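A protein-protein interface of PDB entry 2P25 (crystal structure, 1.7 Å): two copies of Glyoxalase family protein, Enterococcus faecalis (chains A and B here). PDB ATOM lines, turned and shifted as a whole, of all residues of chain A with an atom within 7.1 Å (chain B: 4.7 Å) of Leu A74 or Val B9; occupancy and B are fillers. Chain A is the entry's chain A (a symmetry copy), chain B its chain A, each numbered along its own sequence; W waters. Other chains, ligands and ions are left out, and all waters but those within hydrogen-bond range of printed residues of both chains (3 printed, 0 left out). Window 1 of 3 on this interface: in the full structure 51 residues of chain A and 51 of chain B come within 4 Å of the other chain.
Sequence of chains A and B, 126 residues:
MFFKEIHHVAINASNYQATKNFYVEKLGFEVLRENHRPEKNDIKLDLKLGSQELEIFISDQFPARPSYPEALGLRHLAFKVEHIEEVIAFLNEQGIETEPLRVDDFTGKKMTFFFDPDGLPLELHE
Printed residues of chain B within 4 Å of Ile A6: Leu B77. Of the printed residues of chain B, Leu A74 touches Val B9 (3.3 Å), Ala B10 (3.7 Å), Ile B11 (3.7 Å), Leu B74 (3.3 Å), Arg B75 (3.9 Å), His B76 (3.4 Å), Leu B77 (3.8 Å) and Leu B120 (3.7 Å). Of chain A, only Leu A74, His A76 and Leu A77 come within 4 Å of Val B9. Glu B53 touches none of the printed residues of chain A. Of the printed residues of chain A, Leu B74 touches Val A9, Ala A10, Leu A74, Arg A75, His A76, Leu A77 and Leu A120. Printed residues of chain A within 4 Å of Leu B120: Leu A74 (3.7 Å). The nearest printed residue of chain B that does not touch Leu A74 is Leu B54 (6.3 Å). The nearest residue of chain A that does not touch Val B9 is Val A9 (4.2 Å).
O of Ala B10 lies within hydrogen-bond range of N of Arg A75, at 2.8 Å. The backbone carbonyl oxygen (O) of His B76 lies within hydrogen-bond range of the backbone NH (N) of Ala A10 (3.0 Å). O of Ala A10 lies within hydrogen-bond range of N of Arg B75 (2.8 Å). The backbone NH (N) of Ala B10 lies within hydrogen-bond range of the backbone carbonyl oxygen (O) of His A76, at 3.0 Å. The backbone NH (N) of Ala A78 is in hydrogen-bond range of the backbone carbonyl oxygen (O) of His B8.
Ile A6 touches Leu B77 (CG2 to CD1, 3.9 Å). CA of Val A9 touches O of His B76, 3.8 Å away. Gly A73 touches Ile B11. Ile B11 touches Leu A74. CE1 of His B8 touches CE1 of His A76 (2.8 Å). Leu B74 touches His A76. Leu A77 touches Ile B6. C of Leu A77 touches O of His B8, 3.9 Å away. Leu B74 touches Leu A77. Leu A120 touches Leu B74.
Printed residues of chain A that touch a printed residue of chain B: Ile A6, Val A9, Ala A10, Gly A73, Leu A74, Arg A75, His A76, Leu A77, Ala A78 and Leu A120. Hydrophobic or aromatic side chains of chain A within 4 Å of the printed part of chain B: Ile A6, Val A9, Ala A10, Leu A74, His A76, Leu A77, Ala A78 and Leu A120. Among the printed residues, no Asp or Glu carboxylate lies within 4 Å of a Lys or Arg side-chain nitrogen of the other chain.
Water W2 bridges O of Leu B74 (2.9 Å) and N of Leu A74 (3.0 Å). Water W1 lies within hydrogen-bond range of the backbone carbonyl oxygen of Leu A74, the backbone NH of Leu B74 and the guanidinium group of Arg A65. Water W3 lies within hydrogen-bond range of the backbone NH (N) of Gly A73 (3.1 Å) and the backbone NH (N) of Leu B120 (3.5 Å).
The backbone NH (N) of Val B9 is in hydrogen-bond range of the backbone carbonyl oxygen (O) of Glu B53. N of Ile B11 lies within hydrogen-bond range of O of Glu B55 (2.8 Å). O of Val B9 lies within hydrogen-bond range of N of Glu B55, at 2.9 Å. The backbone carbonyl oxygen of Arg A75 is in hydrogen-bond range of the guanidinium group of Arg A65, at 2.8 Å. NH1 of Arg A75 is in salt-bridge range of OE1 of Glu A70 (3.6 Å).
Ala A10 touches Arg B75, and with the chains exchanged Arg A75 touches Ala B10. Leu B74 touches its own counterpart, Leu A74. Leu A74 touches His B76, and with the chains exchanged His A76 touches Leu B74. Leu A74 touches Leu B77, and with the chains exchanged Leu A77 touches Leu B74. 8 positions are printed for both chains. Of the 30 pairs that touch across the chains among the printed residues, 23 have their exchanged pair printed and touching as well.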
ATOM      1  N   ILE A   6      10.327 -25.506  27.925  1.00  0.00           N
ATOM      2  CA  ILE A   6      10.463 -24.334  27.058  1.00  0.00           C
ATOM      3  C   ILE A   6      11.849 -24.277  26.406  1.00  0.00           C
ATOM      4  O   ILE A   6      12.885 -24.344  27.104  1.00  0.00           O
ATOM      5  CB  ILE A   6      10.189 -23.042  27.838  1.00  0.00           C
ATOM      6  CG1 ILE A   6       8.761 -23.061  28.394  1.00  0.00           C
ATOM      7  CG2 ILE A   6      10.415 -21.794  26.932  1.00  0.00           C
ATOM      8  CD1 ILE A   6       8.429 -21.830  29.260  1.00  0.00           C
ATOM      9  N   VAL A   9      11.568 -18.157  24.643  1.00  0.00           N
ATOM     10  CA  VAL A   9      10.475 -17.226  24.494  1.00  0.00           C
ATOM     11  C   VAL A   9      11.003 -16.171  23.506  1.00  0.00           C
ATOM     12  O   VAL A   9      12.168 -15.803  23.587  1.00  0.00           O
ATOM     13  CB  VAL A   9      10.145 -16.590  25.847  1.00  0.00           C
ATOM     14  CG1 VAL A   9       9.205 -15.435  25.698  1.00  0.00           C
ATOM     15  CG2 VAL A   9       9.508 -17.634  26.776  1.00  0.00           C
ATOM     16  N   ALA A  10      10.188 -15.768  22.536  1.00  0.00           N
ATOM     17  CA  ALA A  10      10.593 -14.739  21.534  1.00  0.00           C
ATOM     18  C   ALA A  10       9.930 -13.394  21.807  1.00  0.00           C
ATOM     19  O   ALA A  10       8.759 -13.328  22.196  1.00  0.00           O
ATOM     20  CB  ALA A  10      10.224 -15.193  20.131  1.00  0.00           C
ATOM     21  N   ARG A  65       3.122  -2.113  21.271  1.00  0.00           N
ATOM     22  CA  ARG A  65       2.436  -3.229  21.908  1.00  0.00           C
ATOM     23  C   ARG A  65       1.031  -2.729  22.311  1.00  0.00           C
ATOM     24  O   ARG A  65       0.901  -1.721  23.010  1.00  0.00           O
ATOM     25  CB  ARG A  65       3.217  -3.635  23.153  1.00  0.00           C
ATOM     26  CG  ARG A  65       2.547  -4.787  23.909  1.00  0.00           C
ATOM     27  CD  ARG A  65       3.319  -5.102  25.192  1.00  0.00           C
ATOM     28  NE  ARG A  65       2.679  -6.181  25.936  1.00  0.00           N
ATOM     29  CZ  ARG A  65       1.724  -6.005  26.845  1.00  0.00           C
ATOM     30  NH1 ARG A  65       1.263  -4.784  27.109  1.00  0.00           N
ATOM     31  NH2 ARG A  65       1.222  -7.064  27.479  1.00  0.00           N
ATOM     32  N   GLU A  70      -5.317  -4.723  26.056  1.00  0.00           N
ATOM     33  CA  GLU A  70      -4.299  -5.611  25.496  1.00  0.00           C
ATOM     34  C   GLU A  70      -4.924  -6.546  24.454  1.00  0.00           C
ATOM     35  O   GLU A  70      -6.134  -6.784  24.438  1.00  0.00           O
ATOM     36  CB  GLU A  70      -3.636  -6.424  26.583  1.00  0.00           C
ATOM     37  CG  GLU A  70      -2.652  -5.631  27.444  1.00  0.00           C
ATOM     38  CD  GLU A  70      -2.018  -6.506  28.495  1.00  0.00           C
ATOM     39  OE1 GLU A  70      -2.564  -7.608  28.720  1.00  0.00           O
ATOM     40  OE2 GLU A  70      -0.989  -6.107  29.099  1.00  0.00           O
ATOM     41  N   ALA A  71      -4.080  -7.075  23.581  1.00  0.00           N
ATOM     42  CA  ALA A  71      -4.570  -7.952  22.543  1.00  0.00           C
ATOM     43  C   ALA A  71      -4.379  -9.416  22.971  1.00  0.00           C
ATOM     44  O   ALA A  71      -3.613  -9.746  23.894  1.00  0.00           O
ATOM     45  CB  ALA A  71      -3.826  -7.679  21.237  1.00  0.00           C
ATOM     46  N   LEU A  72      -5.099 -10.268  22.281  1.00  0.00           N
ATOM     47  CA  LEU A  72      -4.864 -11.702  22.363  1.00  0.00           C
ATOM     48  C   LEU A  72      -3.406 -12.032  22.099  1.00  0.00           C
ATOM     49  O   LEU A  72      -2.724 -11.341  21.308  1.00  0.00           O
ATOM     50  CB  LEU A  72      -5.774 -12.400  21.349  1.00  0.00           C
ATOM     51  CG  LEU A  72      -7.260 -12.295  21.712  1.00  0.00           C
ATOM     52  CD1 LEU A  72      -8.109 -12.700  20.519  1.00  0.00           C
ATOM     53  CD2 LEU A  72      -7.580 -13.169  22.957  1.00  0.00           C
ATOM     54  N   GLY A  73      -2.934 -13.096  22.754  1.00  0.00           N
ATOM     55  CA  GLY A  73      -1.579 -13.610  22.529  1.00  0.00           C
ATOM     56  C   GLY A  73      -0.767 -13.546  23.799  1.00  0.00           C
ATOM     57  O   GLY A  73      -1.302 -13.553  24.897  1.00  0.00           O
ATOM     58  N   LEU A  74       0.550 -13.522  23.660  1.00  0.00           N
ATOM     59  CA  LEU A  74       1.408 -13.494  24.861  1.00  0.00           C
ATOM     60  C   LEU A  74       1.342 -12.133  25.550  1.00  0.00           C
ATOM     61  O   LEU A  74       1.430 -11.095  24.898  1.00  0.00           O
ATOM     62  CB  LEU A  74       2.822 -13.846  24.457  1.00  0.00           C
ATOM     63  CG  LEU A  74       3.023 -15.348  24.196  1.00  0.00           C
ATOM     64  CD1 LEU A  74       4.278 -15.585  23.337  1.00  0.00           C
ATOM     65  CD2 LEU A  74       3.138 -16.085  25.550  1.00  0.00           C
ATOM     66  N   ARG A  75       1.169 -12.159  26.868  1.00  0.00           N
ATOM     67  CA  ARG A  75       0.909 -10.961  27.666  1.00  0.00           C
ATOM     68  C   ARG A  75       2.148 -10.483  28.441  1.00  0.00           C
ATOM     69  O   ARG A  75       2.531  -9.313  28.378  1.00  0.00           O
ATOM     70  CB  ARG A  75      -0.213 -11.285  28.680  1.00  0.00           C
ATOM     71  CG  ARG A  75      -0.560 -10.166  29.633  1.00  0.00           C
ATOM     72  CD  ARG A  75      -1.621 -10.734  30.578  1.00  0.00           C
ATOM     73  NE  ARG A  75      -2.103  -9.806  31.588  1.00  0.00           N
ATOM     74  CZ  ARG A  75      -3.385  -9.429  31.730  1.00  0.00           C
ATOM     75  NH1 ARG A  75      -4.355  -9.835  30.888  1.00  0.00           N
ATOM     76  NH2 ARG A  75      -3.693  -8.597  32.712  1.00  0.00           N
ATOM     77  N   HIS A  76       2.725 -11.374  29.221  1.00  0.00           N
ATOM     78  CA  HIS A  76       3.926 -11.011  30.010  1.00  0.00           C
ATOM     79  C   HIS A  76       4.783 -12.208  30.300  1.00  0.00           C
ATOM     80  O   HIS A  76       4.361 -13.347  30.092  1.00  0.00           O
ATOM     81  CB  HIS A  76       3.578 -10.190  31.271  1.00  0.00           C
ATOM     82  CG  HIS A  76       2.829 -10.948  32.343  1.00  0.00           C
ATOM     83  ND1 HIS A  76       3.363 -12.012  33.033  1.00  0.00           N
ATOM     84  CD2 HIS A  76       1.605 -10.729  32.885  1.00  0.00           C
ATOM     85  CE1 HIS A  76       2.493 -12.436  33.938  1.00  0.00           C
ATOM     86  NE2 HIS A  76       1.409 -11.688  33.847  1.00  0.00           N
ATOM     87  N   LEU A  77       6.002 -11.946  30.791  1.00  0.00           N
ATOM     88  CA  LEU A  77       6.911 -13.003  31.190  1.00  0.00           C
ATOM     89  C   LEU A  77       7.243 -12.734  32.645  1.00  0.00           C
ATOM     90  O   LEU A  77       7.453 -11.584  33.003  1.00  0.00           O
ATOM     91  CB  LEU A  77       8.207 -12.890  30.384  1.00  0.00           C
ATOM     92  CG  LEU A  77       9.337 -13.857  30.647  1.00  0.00           C
ATOM     93  CD1 LEU A  77       8.870 -15.299  30.469  1.00  0.00           C
ATOM     94  CD2 LEU A  77      10.465 -13.518  29.628  1.00  0.00           C
ATOM     95  N   ALA A  78       7.211 -13.771  33.479  1.00  0.00           N
ATOM     96  CA  ALA A  78       7.431 -13.585  34.918  1.00  0.00           C
ATOM     97  C   ALA A  78       8.669 -14.326  35.354  1.00  0.00           C
ATOM     98  O   ALA A  78       8.843 -15.493  34.980  1.00  0.00           O
ATOM     99  CB  ALA A  78       6.229 -14.112  35.679  1.00  0.00           C
ATOM    100  N   LEU A 120       7.164  -3.840  27.322  1.00  0.00           N
ATOM    101  CA  LEU A 120       6.761  -5.217  27.613  1.00  0.00           C
ATOM    102  C   LEU A 120       6.734  -5.407  29.121  1.00  0.00           C
ATOM    103  O   LEU A 120       7.752  -5.160  29.774  1.00  0.00           O
ATOM    104  CB  LEU A 120       7.742  -6.230  27.009  1.00  0.00           C
ATOM    105  CG  LEU A 120       7.396  -7.709  27.289  1.00  0.00           C
ATOM    106  CD1 LEU A 120       5.963  -8.126  26.794  1.00  0.00           C
ATOM    107  CD2 LEU A 120       8.465  -8.594  26.674  1.00  0.00           C
ATOM    108  N   ILE B   6      12.259 -18.713  34.975  1.00  0.00           N
ATOM    109  CA  ILE B   6      10.898 -18.292  34.643  1.00  0.00           C
ATOM    110  C   ILE B   6       9.881 -18.830  35.658  1.00  0.00           C
ATOM    111  O   ILE B   6       9.837 -20.050  35.928  1.00  0.00           O
ATOM    112  CB  ILE B   6      10.518 -18.735  33.224  1.00  0.00           C
ATOM    113  CG1 ILE B   6      11.473 -18.102  32.207  1.00  0.00           C
ATOM    114  CG2 ILE B   6       9.039 -18.357  32.907  1.00  0.00           C
ATOM    115  CD1 ILE B   6      11.210 -18.560  30.759  1.00  0.00           C
ATOM    116  N   HIS B   8       6.489 -17.988  35.240  1.00  0.00           N
ATOM    117  CA  HIS B   8       5.417 -18.348  34.312  1.00  0.00           C
ATOM    118  C   HIS B   8       5.473 -17.465  33.081  1.00  0.00           C
ATOM    119  O   HIS B   8       6.165 -16.430  33.056  1.00  0.00           O
ATOM    120  CB  HIS B   8       4.029 -18.247  34.977  1.00  0.00           C
ATOM    121  CG  HIS B   8       3.658 -16.873  35.461  1.00  0.00           C
ATOM    122  ND1 HIS B   8       3.023 -15.941  34.670  1.00  0.00           N
ATOM    123  CD2 HIS B   8       3.795 -16.297  36.678  1.00  0.00           C
ATOM    124  CE1 HIS B   8       2.808 -14.837  35.368  1.00  0.00           C
ATOM    125  NE2 HIS B   8       3.265 -15.029  36.593  1.00  0.00           N
ATOM    126  N   VAL B   9       4.697 -17.851  32.078  1.00  0.00           N
ATOM    127  CA  VAL B   9       4.446 -17.037  30.913  1.00  0.00           C
ATOM    128  C   VAL B   9       2.926 -16.802  30.932  1.00  0.00           C
ATOM    129  O   VAL B   9       2.181 -17.717  31.262  1.00  0.00           O
ATOM    130  CB  VAL B   9       4.867 -17.791  29.650  1.00  0.00           C
ATOM    131  CG1 VAL B   9       4.388 -17.102  28.412  1.00  0.00           C
ATOM    132  CG2 VAL B   9       6.398 -17.908  29.594  1.00  0.00           C
ATOM    133  N   ALA B  10       2.484 -15.574  30.675  1.00  0.00           N
ATOM    134  CA  ALA B  10       1.030 -15.241  30.651  1.00  0.00           C
ATOM    135  C   ALA B  10       0.516 -15.057  29.228  1.00  0.00           C
ATOM    136  O   ALA B  10       1.206 -14.498  28.368  1.00  0.00           O
ATOM    137  CB  ALA B  10       0.768 -13.966  31.436  1.00  0.00           C
ATOM    138  N   ILE B  11      -0.717 -15.506  28.998  1.00  0.00           N
ATOM    139  CA  ILE B  11      -1.347 -15.489  27.659  1.00  0.00           C
ATOM    140  C   ILE B  11      -2.735 -14.909  27.829  1.00  0.00           C
ATOM    141  O   ILE B  11      -3.399 -15.182  28.821  1.00  0.00           O
ATOM    142  CB  ILE B  11      -1.457 -16.949  27.102  1.00  0.00           C
ATOM    143  CG1 ILE B  11      -0.061 -17.465  26.726  1.00  0.00           C
ATOM    144  CG2 ILE B  11      -2.428 -17.035  25.885  1.00  0.00           C
ATOM    145  CD1 ILE B  11      -0.029 -19.026  26.627  1.00  0.00           C
ATOM    146  N   GLU B  53       4.911 -23.139  34.321  1.00  0.00           N
ATOM    147  CA  GLU B  53       3.593 -22.584  34.640  1.00  0.00           C
ATOM    148  C   GLU B  53       3.101 -21.640  33.555  1.00  0.00           C
ATOM    149  O   GLU B  53       3.869 -20.846  32.992  1.00  0.00           O
ATOM    150  CB  GLU B  53       3.613 -21.896  35.997  1.00  0.00           C
ATOM    151  CG  GLU B  53       2.260 -21.395  36.480  1.00  0.00           C
ATOM    152  CD  GLU B  53       2.214 -21.217  38.007  1.00  0.00           C
ATOM    153  OE1 GLU B  53       2.970 -21.913  38.727  1.00  0.00           O
ATOM    154  OE2 GLU B  53       1.413 -20.381  38.479  1.00  0.00           O
ATOM    155  N   LEU B  54       1.815 -21.750  33.253  1.00  0.00           N
ATOM    156  CA  LEU B  54       1.212 -20.930  32.219  1.00  0.00           C
ATOM    157  C   LEU B  54       0.017 -20.235  32.840  1.00  0.00           C
ATOM    158  O   LEU B  54      -0.831 -20.894  33.440  1.00  0.00           O
ATOM    159  CB  LEU B  54       0.778 -21.843  31.066  1.00  0.00           C
ATOM    160  CG  LEU B  54       0.832 -21.425  29.627  1.00  0.00           C
ATOM    161  CD1 LEU B  54       2.277 -21.091  29.207  1.00  0.00           C
ATOM    162  CD2 LEU B  54       0.243 -22.569  28.816  1.00  0.00           C
ATOM    163  N   GLU B  55      -0.030 -18.913  32.756  1.00  0.00           N
ATOM    164  CA  GLU B  55      -1.138 -18.121  33.284  1.00  0.00           C
ATOM    165  C   GLU B  55      -1.983 -17.588  32.144  1.00  0.00           C
ATOM    166  O   GLU B  55      -1.476 -16.841  31.312  1.00  0.00           O
ATOM    167  CB  GLU B  55      -0.549 -16.962  34.039  1.00  0.00           C
ATOM    168  CG  GLU B  55      -1.462 -16.130  34.829  1.00  0.00           C
ATOM    169  CD  GLU B  55      -0.670 -15.341  35.847  1.00  0.00           C
ATOM    170  OE1 GLU B  55      -0.243 -15.921  36.888  1.00  0.00           O
ATOM    171  OE2 GLU B  55      -0.452 -14.156  35.584  1.00  0.00           O
ATOM    172  N   LEU B  74       5.832  -9.649  23.402  1.00  0.00           N
ATOM    173  CA  LEU B  74       6.070 -11.101  23.272  1.00  0.00           C
ATOM    174  C   LEU B  74       5.499 -11.634  21.960  1.00  0.00           C
ATOM    175  O   LEU B  74       4.369 -11.320  21.594  1.00  0.00           O
ATOM    176  CB  LEU B  74       5.466 -11.802  24.468  1.00  0.00           C
ATOM    177  CG  LEU B  74       6.307 -11.653  25.747  1.00  0.00           C
ATOM    178  CD1 LEU B  74       5.449 -11.931  26.994  1.00  0.00           C
ATOM    179  CD2 LEU B  74       7.507 -12.624  25.678  1.00  0.00           C
ATOM    180  N   ARG B  75       6.302 -12.428  21.259  1.00  0.00           N
ATOM    181  CA  ARG B  75       5.994 -12.887  19.905  1.00  0.00           C
ATOM    182  C   ARG B  75       5.510 -14.346  19.869  1.00  0.00           C
ATOM    183  O   ARG B  75       4.469 -14.662  19.288  1.00  0.00           O
ATOM    184  CB  ARG B  75       7.275 -12.770  19.046  1.00  0.00           C
ATOM    185  CG  ARG B  75       7.145 -13.268  17.627  1.00  0.00           C
ATOM    186  CD  ARG B  75       8.535 -13.129  17.004  1.00  0.00           C
ATOM    187  NE  ARG B  75       8.633 -13.557  15.619  1.00  0.00           N
ATOM    188  CZ  ARG B  75       9.018 -12.771  14.600  1.00  0.00           C
ATOM    189  NH1 ARG B  75       9.294 -11.462  14.763  1.00  0.00           N
ATOM    190  NH2 ARG B  75       9.091 -13.297  13.388  1.00  0.00           N
ATOM    191  N   HIS B  76       6.304 -15.236  20.428  1.00  0.00           N
ATOM    192  CA  HIS B  76       5.926 -16.669  20.444  1.00  0.00           C
ATOM    193  C   HIS B  76       6.550 -17.394  21.601  1.00  0.00           C
ATOM    194  O   HIS B  76       7.441 -16.864  22.267  1.00  0.00           O
ATOM    195  CB  HIS B  76       6.175 -17.360  19.086  1.00  0.00           C
ATOM    196  CG  HIS B  76       7.629 -17.518  18.702  1.00  0.00           C
ATOM    197  ND1 HIS B  76       8.517 -18.301  19.403  1.00  0.00           N
ATOM    198  CD2 HIS B  76       8.315 -17.038  17.635  1.00  0.00           C
ATOM    199  CE1 HIS B  76       9.697 -18.280  18.802  1.00  0.00           C
ATOM    200  NE2 HIS B  76       9.604 -17.499  17.741  1.00  0.00           N
ATOM    201  N   LEU B  77       6.076 -18.625  21.839  1.00  0.00           N
ATOM    202  CA  LEU B  77       6.635 -19.474  22.873  1.00  0.00           C
ATOM    203  C   LEU B  77       7.074 -20.745  22.173  1.00  0.00           C
ATOM    204  O   LEU B  77       6.352 -21.228  21.313  1.00  0.00           O
ATOM    205  CB  LEU B  77       5.538 -19.845  23.874  1.00  0.00           C
ATOM    206  CG  LEU B  77       5.859 -20.763  25.030  1.00  0.00           C
ATOM    207  CD1 LEU B  77       7.002 -20.199  25.868  1.00  0.00           C
ATOM    208  CD2 LEU B  77       4.562 -20.881  25.883  1.00  0.00           C
ATOM    209  N   LEU B 120      -2.090 -17.633  18.461  1.00  0.00           N
ATOM    210  CA  LEU B 120      -0.770 -17.447  19.066  1.00  0.00           C
ATOM    211  C   LEU B 120       0.186 -18.465  18.468  1.00  0.00           C
ATOM    212  O   LEU B 120      -0.098 -19.664  18.532  1.00  0.00           O
ATOM    213  CB  LEU B 120      -0.814 -17.651  20.586  1.00  0.00           C
ATOM    214  CG  LEU B 120       0.547 -17.490  21.299  1.00  0.00           C
ATOM    215  CD1 LEU B 120       1.225 -16.093  21.055  1.00  0.00           C
ATOM    216  CD2 LEU B 120       0.366 -17.759  22.782  1.00  0.00           C
HETATM  217  O   HOH W   1       3.117  -8.838  24.327  1.00  0.00           O
HETATM  218  O   HOH W   2       1.692 -12.291  21.197  1.00  0.00           O
HETATM  219  O   HOH W   3      -3.236 -14.850  20.164  1.00  0.00           O
